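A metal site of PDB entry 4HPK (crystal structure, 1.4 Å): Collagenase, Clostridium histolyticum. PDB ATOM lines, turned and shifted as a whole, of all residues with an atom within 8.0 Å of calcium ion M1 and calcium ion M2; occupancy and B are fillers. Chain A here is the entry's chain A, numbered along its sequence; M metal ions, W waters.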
ATOM      1  N   GLU A   4      -2.678  -3.073  26.007  1.00  0.00           N
ATOM      2  CA  GLU A   4      -3.371  -4.359  25.909  1.00  0.00           C
ATOM      3  C   GLU A   4      -4.857  -4.213  26.170  1.00  0.00           C
ATOM      4  O   GLU A   4      -5.298  -3.219  26.776  1.00  0.00           O
ATOM      5  CB  GLU A   4      -2.780  -5.344  26.906  1.00  0.00           C
ATOM      6  CG  GLU A   4      -2.954  -4.863  28.354  1.00  0.00           C
ATOM      7  CD  GLU A   4      -2.656  -5.928  29.397  1.00  0.00           C
ATOM      8  OE1 GLU A   4      -2.956  -7.117  29.161  1.00  0.00           O
ATOM      9  OE2 GLU A   4      -2.155  -5.557  30.469  1.00  0.00           O
ATOM     10  N   LYS A   5      -5.622  -5.215  25.747  1.00  0.00           N
ATOM     11  CA  LYS A   5      -7.066  -5.219  25.937  1.00  0.00           C
ATOM     12  C   LYS A   5      -7.496  -6.476  26.712  1.00  0.00           C
ATOM     13  O   LYS A   5      -7.552  -7.558  26.155  1.00  0.00           O
ATOM     14  CB  LYS A   5      -7.781  -5.158  24.579  1.00  0.00           C
ATOM     15  CG  LYS A   5      -7.527  -3.871  23.793  1.00  0.00           C
ATOM     16  CD  LYS A   5      -8.368  -3.806  22.528  1.00  0.00           C
ATOM     17  CE  LYS A   5      -7.934  -2.661  21.622  1.00  0.00           C
ATOM     18  NZ  LYS A   5      -7.937  -1.350  22.335  1.00  0.00           N
ATOM     19  N   GLU A   6      -7.793  -6.320  28.004  1.00  0.00           N
ATOM     20  CA  GLU A   6      -8.338  -7.428  28.788  1.00  0.00           C
ATOM     21  C   GLU A   6      -9.800  -7.646  28.426  1.00  0.00           C
ATOM     22  O   GLU A   6     -10.459  -6.699  28.007  1.00  0.00           O
ATOM     23  CB  GLU A   6      -8.220  -7.170  30.288  1.00  0.00           C
ATOM     24  CG  GLU A   6      -6.800  -7.127  30.817  1.00  0.00           C
ATOM     25  CD  GLU A   6      -6.102  -8.475  30.868  1.00  0.00           C
ATOM     26  OE1 GLU A   6      -6.742  -9.537  30.698  1.00  0.00           O
ATOM     27  OE2 GLU A   6      -4.879  -8.464  31.099  1.00  0.00           O
ATOM     28  N   ASN A   7     -10.323  -8.859  28.548  1.00  0.00           N
ATOM     29  CA  ASN A   7      -9.591 -10.080  28.915  1.00  0.00           C
ATOM     30  C   ASN A   7      -8.836 -10.635  27.714  1.00  0.00           C
ATOM     31  O   ASN A   7      -9.416 -10.787  26.635  1.00  0.00           O
ATOM     32  CB  ASN A   7     -10.616 -11.119  29.414  1.00  0.00           C
ATOM     33  CG  ASN A   7      -9.961 -12.341  29.981  1.00  0.00           C
ATOM     34  OD1 ASN A   7      -9.222 -13.044  29.288  1.00  0.00           O
ATOM     35  ND2 ASN A   7     -10.268 -12.650  31.235  1.00  0.00           N
ATOM     36  N   ASN A   8      -7.550 -10.939  27.915  1.00  0.00           N
ATOM     37  CA  ASN A   8      -6.688 -11.509  26.874  1.00  0.00           C
ATOM     38  C   ASN A   8      -5.950 -12.749  27.368  1.00  0.00           C
ATOM     39  O   ASN A   8      -4.824 -13.023  26.992  1.00  0.00           O
ATOM     40  CB  ASN A   8      -5.704 -10.446  26.356  1.00  0.00           C
ATOM     41  CG  ASN A   8      -4.812  -9.901  27.452  1.00  0.00           C
ATOM     42  OD1 ASN A   8      -4.795 -10.425  28.559  1.00  0.00           O
ATOM     43  ND2 ASN A   8      -4.109  -8.824  27.164  1.00  0.00           N
ATOM     44  N   ASP A   9      -6.628 -13.550  28.188  1.00  0.00           N
ATOM     45  CA  ASP A   9      -5.956 -14.631  28.903  1.00  0.00           C
ATOM     46  C   ASP A   9      -5.801 -15.922  28.069  1.00  0.00           C
ATOM     47  O   ASP A   9      -5.132 -16.873  28.516  1.00  0.00           O
ATOM     48  CB  ASP A   9      -6.686 -14.915  30.218  1.00  0.00           C
ATOM     49  CG  ASP A   9      -6.578 -13.758  31.231  1.00  0.00           C
ATOM     50  OD1 ASP A   9      -7.126 -13.940  32.330  1.00  0.00           O
ATOM     51  OD2 ASP A   9      -5.973 -12.691  30.957  1.00  0.00           O
ATOM     52  N   SER A  10      -6.396 -15.969  26.885  1.00  0.00           N
ATOM     53  CA  SER A  10      -6.287 -17.106  25.970  1.00  0.00           C
ATOM     54  C   SER A  10      -6.054 -16.607  24.547  1.00  0.00           C
ATOM     55  O   SER A  10      -6.320 -15.439  24.263  1.00  0.00           O
ATOM     56  CB  SER A  10      -7.549 -17.967  26.036  1.00  0.00           C
ATOM     57  OG  SER A  10      -8.681 -17.175  25.747  1.00  0.00           O
ATOM     58  N   LYS A  13      -8.615 -14.720  22.522  1.00  0.00           N
ATOM     59  CA  LYS A  13      -8.866 -13.382  23.047  1.00  0.00           C
ATOM     60  C   LYS A  13      -7.616 -12.509  22.965  1.00  0.00           C
ATOM     61  O   LYS A  13      -7.534 -11.491  23.630  1.00  0.00           O
ATOM     62  CB  LYS A  13      -9.329 -13.487  24.504  1.00  0.00           C
ATOM     63  CG  LYS A  13     -10.740 -14.084  24.671  1.00  0.00           C
ATOM     64  CD  LYS A  13     -11.080 -14.357  26.132  1.00  0.00           C
ATOM     65  CE  LYS A  13     -12.402 -15.126  26.261  1.00  0.00           C
ATOM     66  NZ  LYS A  13     -12.560 -15.772  27.598  1.00  0.00           N
ATOM     67  N   THR A  15      -4.650  -9.895  22.269  1.00  0.00           N
ATOM     68  CA  THR A  15      -4.583  -8.501  21.848  1.00  0.00           C
ATOM     69  C   THR A  15      -3.713  -8.423  20.586  1.00  0.00           C
ATOM     70  O   THR A  15      -2.579  -8.883  20.586  1.00  0.00           O
ATOM     71  CB  THR A  15      -3.969  -7.600  22.921  1.00  0.00           C
ATOM     72  OG1 THR A  15      -4.749  -7.672  24.130  1.00  0.00           O
ATOM     73  CG2 THR A  15      -3.890  -6.151  22.436  1.00  0.00           C
ATOM     74  N   GLN A  25       1.801  -1.389  25.957  1.00  0.00           N
ATOM     75  CA  GLN A  25       1.861  -1.300  27.421  1.00  0.00           C
ATOM     76  C   GLN A  25       0.953  -2.335  28.053  1.00  0.00           C
ATOM     77  O   GLN A  25      -0.162  -2.537  27.607  1.00  0.00           O
ATOM     78  CB  GLN A  25       1.424   0.089  27.898  1.00  0.00           C
ATOM     79  CG  GLN A  25       2.378   1.202  27.488  1.00  0.00           C
ATOM     80  CD  GLN A  25       2.078   2.519  28.178  1.00  0.00           C
ATOM     81  OE1 GLN A  25       0.918   2.919  28.269  1.00  0.00           O
ATOM     82  NE2 GLN A  25       3.117   3.187  28.661  1.00  0.00           N
ATOM     83  N   GLY A  26       1.463  -3.034  29.054  1.00  0.00           N
ATOM     84  CA  GLY A  26       0.651  -4.008  29.749  1.00  0.00           C
ATOM     85  C   GLY A  26       0.999  -4.129  31.208  1.00  0.00           C
ATOM     86  O   GLY A  26       1.957  -3.547  31.702  1.00  0.00           O
ATOM     87  N   SER A  27       0.198  -4.913  31.907  1.00  0.00           N
ATOM     88  CA  SER A  27       0.444  -5.202  33.316  1.00  0.00           C
ATOM     89  C   SER A  27       0.017  -6.612  33.630  1.00  0.00           C
ATOM     90  O   SER A  27      -0.900  -7.123  32.998  1.00  0.00           O
ATOM     91  CB  SER A  27      -0.286  -4.218  34.222  1.00  0.00           C
ATOM     92  OG  SER A  27      -1.673  -4.459  34.220  1.00  0.00           O
ATOM     93  N   LEU A  28       0.719  -7.218  34.602  1.00  0.00           N
ATOM     94  CA  LEU A  28       0.349  -8.524  35.148  1.00  0.00           C
ATOM     95  C   LEU A  28       0.309  -8.393  36.668  1.00  0.00           C
ATOM     96  O   LEU A  28       1.223  -8.798  37.375  1.00  0.00           O
ATOM     97  CB  LEU A  28       1.363  -9.603  34.737  1.00  0.00           C
ATOM     98  CG  LEU A  28       1.333  -9.958  33.245  1.00  0.00           C
ATOM     99  CD1 LEU A  28       2.550 -10.805  32.881  1.00  0.00           C
ATOM    100  CD2 LEU A  28       0.069 -10.654  32.866  1.00  0.00           C
ATOM    101  N   LEU A  29      -0.776  -7.784  37.146  1.00  0.00           N
ATOM    102  CA  LEU A  29      -0.928  -7.467  38.578  1.00  0.00           C
ATOM    103  C   LEU A  29      -1.854  -8.479  39.227  1.00  0.00           C
ATOM    104  O   LEU A  29      -2.893  -8.798  38.676  1.00  0.00           O
ATOM    105  CB  LEU A  29      -1.519  -6.073  38.765  1.00  0.00           C
ATOM    106  CG  LEU A  29      -0.821  -4.974  37.960  1.00  0.00           C
ATOM    107  CD1 LEU A  29      -1.602  -3.667  38.099  1.00  0.00           C
ATOM    108  CD2 LEU A  29       0.642  -4.800  38.372  1.00  0.00           C
ATOM    109  N   ASP A  31      -3.940 -11.507  40.219  1.00  0.00           N
ATOM    110  CA  ASP A  31      -4.344 -12.735  39.551  1.00  0.00           C
ATOM    111  C   ASP A  31      -4.441 -12.614  38.033  1.00  0.00           C
ATOM    112  O   ASP A  31      -4.832 -13.570  37.361  1.00  0.00           O
ATOM    113  CB  ASP A  31      -5.603 -13.365  40.198  1.00  0.00           C
ATOM    114  CG  ASP A  31      -6.862 -12.562  39.957  1.00  0.00           C
ATOM    115  OD1 ASP A  31      -6.884 -11.664  39.105  1.00  0.00           O
ATOM    116  OD2 ASP A  31      -7.873 -12.849  40.670  1.00  0.00           O
ATOM    117  N   ASP A  32      -4.037 -11.475  37.466  1.00  0.00           N
ATOM    118  CA  ASP A  32      -3.829 -11.387  36.028  1.00  0.00           C
ATOM    119  C   ASP A  32      -2.422 -11.872  35.747  1.00  0.00           C
ATOM    120  O   ASP A  32      -1.462 -11.144  35.955  1.00  0.00           O
ATOM    121  CB  ASP A  32      -4.028  -9.947  35.539  1.00  0.00           C
ATOM    122  CG  ASP A  32      -3.845  -9.801  34.040  1.00  0.00           C
ATOM    123  OD1 ASP A  32      -4.288 -10.700  33.280  1.00  0.00           O
ATOM    124  OD2 ASP A  32      -3.268  -8.759  33.597  1.00  0.00           O
ATOM    125  N   SER A  33      -2.300 -13.125  35.316  1.00  0.00           N
ATOM    126  CA  SER A  33      -0.970 -13.724  35.169  1.00  0.00           C
ATOM    127  C   SER A  33      -0.573 -14.042  33.744  1.00  0.00           C
ATOM    128  O   SER A  33       0.565 -14.466  33.533  1.00  0.00           O
ATOM    129  CB  SER A  33      -0.844 -14.983  36.006  1.00  0.00           C
ATOM    130  OG  SER A  33      -1.787 -15.887  35.582  1.00  0.00           O
ATOM    131  N   ARG A  34      -1.475 -13.822  32.794  1.00  0.00           N
ATOM    132  CA  ARG A  34      -1.266 -14.143  31.369  1.00  0.00           C
ATOM    133  C   ARG A  34      -1.859 -13.030  30.518  1.00  0.00           C
ATOM    134  O   ARG A  34      -3.013 -12.626  30.740  1.00  0.00           O
ATOM    135  CB  ARG A  34      -1.987 -15.442  31.011  1.00  0.00           C
ATOM    136  CG  ARG A  34      -1.467 -16.639  31.773  1.00  0.00           C
ATOM    137  CD  ARG A  34      -2.436 -17.755  31.738  1.00  0.00           C
ATOM    138  NE  ARG A  34      -2.786 -18.155  30.374  1.00  0.00           N
ATOM    139  CZ  ARG A  34      -2.233 -19.172  29.711  1.00  0.00           C
ATOM    140  NH1 ARG A  34      -1.253 -19.907  30.249  1.00  0.00           N
ATOM    141  NH2 ARG A  34      -2.676 -19.452  28.490  1.00  0.00           N
ATOM    142  N   ASP A  35      -1.067 -12.543  29.558  1.00  0.00           N
ATOM    143  CA  ASP A  35      -1.541 -11.602  28.548  1.00  0.00           C
ATOM    144  C   ASP A  35      -1.157 -12.177  27.176  1.00  0.00           C
ATOM    145  O   ASP A  35       0.037 -12.249  26.859  1.00  0.00           O
ATOM    146  CB  ASP A  35      -0.900 -10.212  28.704  1.00  0.00           C
ATOM    147  CG  ASP A  35      -1.352  -9.483  29.961  1.00  0.00           C
ATOM    148  OD1 ASP A  35      -2.408  -9.809  30.528  1.00  0.00           O
ATOM    149  OD2 ASP A  35      -0.654  -8.526  30.364  1.00  0.00           O
ATOM    150  N   TYR A  36      -2.147 -12.602  26.404  1.00  0.00           N
ATOM    151  CA  TYR A  36      -1.909 -13.106  25.033  1.00  0.00           C
ATOM    152  C   TYR A  36      -1.972 -12.000  24.021  1.00  0.00           C
ATOM    153  O   TYR A  36      -2.862 -11.153  24.069  1.00  0.00           O
ATOM    154  CB  TYR A  36      -2.908 -14.199  24.651  1.00  0.00           C
ATOM    155  CG  TYR A  36      -2.295 -15.571  24.386  1.00  0.00           C
ATOM    156  CD1 TYR A  36      -2.702 -16.680  25.084  1.00  0.00           C
ATOM    157  CD2 TYR A  36      -1.308 -15.734  23.435  1.00  0.00           C
ATOM    158  CE1 TYR A  36      -2.145 -17.914  24.847  1.00  0.00           C
ATOM    159  CE2 TYR A  36      -0.745 -16.966  23.190  1.00  0.00           C
ATOM    160  CZ  TYR A  36      -1.166 -18.049  23.896  1.00  0.00           C
ATOM    161  OH  TYR A  36      -0.581 -19.282  23.629  1.00  0.00           O
ATOM    162  N   TYR A  37      -0.999 -12.018  23.098  1.00  0.00           N
ATOM    163  CA  TYR A  37      -0.954 -11.116  21.962  1.00  0.00           C
ATOM    164  C   TYR A  37      -0.828 -11.939  20.672  1.00  0.00           C
ATOM    165  O   TYR A  37      -0.474 -13.117  20.714  1.00  0.00           O
ATOM    166  CB  TYR A  37       0.283 -10.223  22.048  1.00  0.00           C
ATOM    167  CG  TYR A  37       0.301  -9.309  23.248  1.00  0.00           C
ATOM    168  CD1 TYR A  37       0.818  -9.720  24.474  1.00  0.00           C
ATOM    169  CD2 TYR A  37      -0.202  -8.032  23.141  1.00  0.00           C
ATOM    170  CE1 TYR A  37       0.841  -8.835  25.567  1.00  0.00           C
ATOM    171  CE2 TYR A  37      -0.180  -7.171  24.207  1.00  0.00           C
ATOM    172  CZ  TYR A  37       0.325  -7.570  25.417  1.00  0.00           C
ATOM    173  OH  TYR A  37       0.316  -6.645  26.442  1.00  0.00           O
ATOM    174  N   LEU A  97       2.529 -15.280  24.199  1.00  0.00           N
ATOM    175  CA  LEU A  97       1.988 -15.330  25.541  1.00  0.00           C
ATOM    176  C   LEU A  97       2.993 -14.697  26.472  1.00  0.00           C
ATOM    177  O   LEU A  97       4.079 -15.238  26.640  1.00  0.00           O
ATOM    178  CB  LEU A  97       1.746 -16.789  25.960  1.00  0.00           C
ATOM    179  CG  LEU A  97       1.319 -17.024  27.415  1.00  0.00           C
ATOM    180  CD1 LEU A  97       0.018 -16.288  27.738  1.00  0.00           C
ATOM    181  CD2 LEU A  97       1.174 -18.513  27.661  1.00  0.00           C
ATOM    182  N   VAL A  98       2.613 -13.572  27.087  1.00  0.00           N
ATOM    183  CA  VAL A  98       3.412 -12.961  28.143  1.00  0.00           C
ATOM    184  C   VAL A  98       2.811 -13.456  29.448  1.00  0.00           C
ATOM    185  O   VAL A  98       1.596 -13.332  29.657  1.00  0.00           O
ATOM    186  CB  VAL A  98       3.370 -11.419  28.079  1.00  0.00           C
ATOM    187  CG1 VAL A  98       4.115 -10.810  29.255  1.00  0.00           C
ATOM    188  CG2 VAL A  98       3.929 -10.924  26.728  1.00  0.00           C
ATOM    189  N   GLY A 105       3.704  -6.883  38.231  1.00  0.00           N
ATOM    190  CA  GLY A 105       4.221  -5.639  37.719  1.00  0.00           C
ATOM    191  C   GLY A 105       3.749  -5.268  36.339  1.00  0.00           C
ATOM    192  O   GLY A 105       2.942  -5.958  35.726  1.00  0.00           O
ATOM    193  N   TYR A 107       4.833  -3.738  32.339  1.00  0.00           N
ATOM    194  CA  TYR A 107       5.841  -4.021  31.322  1.00  0.00           C
ATOM    195  C   TYR A 107       5.494  -3.295  30.022  1.00  0.00           C
ATOM    196  O   TYR A 107       4.367  -2.842  29.829  1.00  0.00           O
ATOM    197  CB  TYR A 107       5.970  -5.538  31.057  1.00  0.00           C
ATOM    198  CG  TYR A 107       4.713  -6.153  30.465  1.00  0.00           C
ATOM    199  CD1 TYR A 107       4.519  -6.182  29.076  1.00  0.00           C
ATOM    200  CD2 TYR A 107       3.701  -6.670  31.265  1.00  0.00           C
ATOM    201  CE1 TYR A 107       3.363  -6.703  28.520  1.00  0.00           C
ATOM    202  CE2 TYR A 107       2.544  -7.185  30.721  1.00  0.00           C
ATOM    203  CZ  TYR A 107       2.389  -7.215  29.354  1.00  0.00           C
ATOM    204  OH  TYR A 107       1.250  -7.731  28.796  1.00  0.00           O
HETATM  205 CA    CA M   1      -4.515 -10.849  30.886  1.00  0.00          CA
HETATM  206 CA    CA M   2      -2.731  -7.617  31.594  1.00  0.00          CA
HETATM  207  O   HOH W   1      -3.917  -5.849  32.718  1.00  0.00           O
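O of Gln 25 sits at hydrogen-bond distance from N of Glu 4 (3.0 Å). The side-chain carboxylate (OD2) of Asp 35 lies close to the side-chain hydroxyl (OH) of Tyr 107. The backbone NH (N) of Asp 35 lies within hydrogen-bond range of the backbone carbonyl oxygen (O) of Val 98, at 2.8 Å. The side-chain amide oxygen (OD1) of Asn 7 is in hydrogen-bond range of the backbone NH (N) of Asp 9 (2.9 Å). The backbone carbonyl oxygen (O) of Asn 8 sits at hydrogen-bond distance from the backbone NH (N) of Tyr 36, 2.8 Å away. ND2 of Asn 8 sits at hydrogen-bond distance from OG1 of Thr 15, at 3.3 Å. ND2 of Asn 8 lies close to OE1 of Glu 4 (2.9 Å).
Within 4 Å of calcium ion M1: Glu 6, Asn 8, Asp 9, Asp 32, Arg 34 and Asp 35. The nearest printed residue that does not touch calcium ion M1 is Glu 4 (4.4 Å).
Five residues have an atom within 4 Å of calcium ion M2: Glu 4, Glu 6, Ser 27, Asp 32 and Asp 35.
Calcium ion M1 is bound by O of Arg 34 (2.3 Å), OD2 of Asp 9 (2.4 Å), OD1 of Asp 35 (2.4 Å), OD1 of Asn 8 (2.4 Å), OD1 of Asp 32 (2.4 Å), OE2 of Glu 6 (2.4 Å) and OE1 of Glu 6 (2.6 Å).
Calcium ion M2 is bound by the backbone carbonyl oxygen (O) of Ser 27 (2.4 Å), the side-chain carboxylate (OE2) of Glu 6 (2.4 Å), the side-chain carboxylate (OD2) of Asp 32 (2.4 Å), water W1 (2.4 Å), the side-chain carboxylate (OE2) of Glu 4 (2.4 Å), the side-chain carboxylate (OD1) of Asp 35 (2.5 Å), the side-chain carboxylate (OE1) of Glu 4 (2.5 Å) and the side-chain carboxylate (OD2) of Asp 35 (2.6 Å). Calcium ion M2 has eight donor atoms within binding distance.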
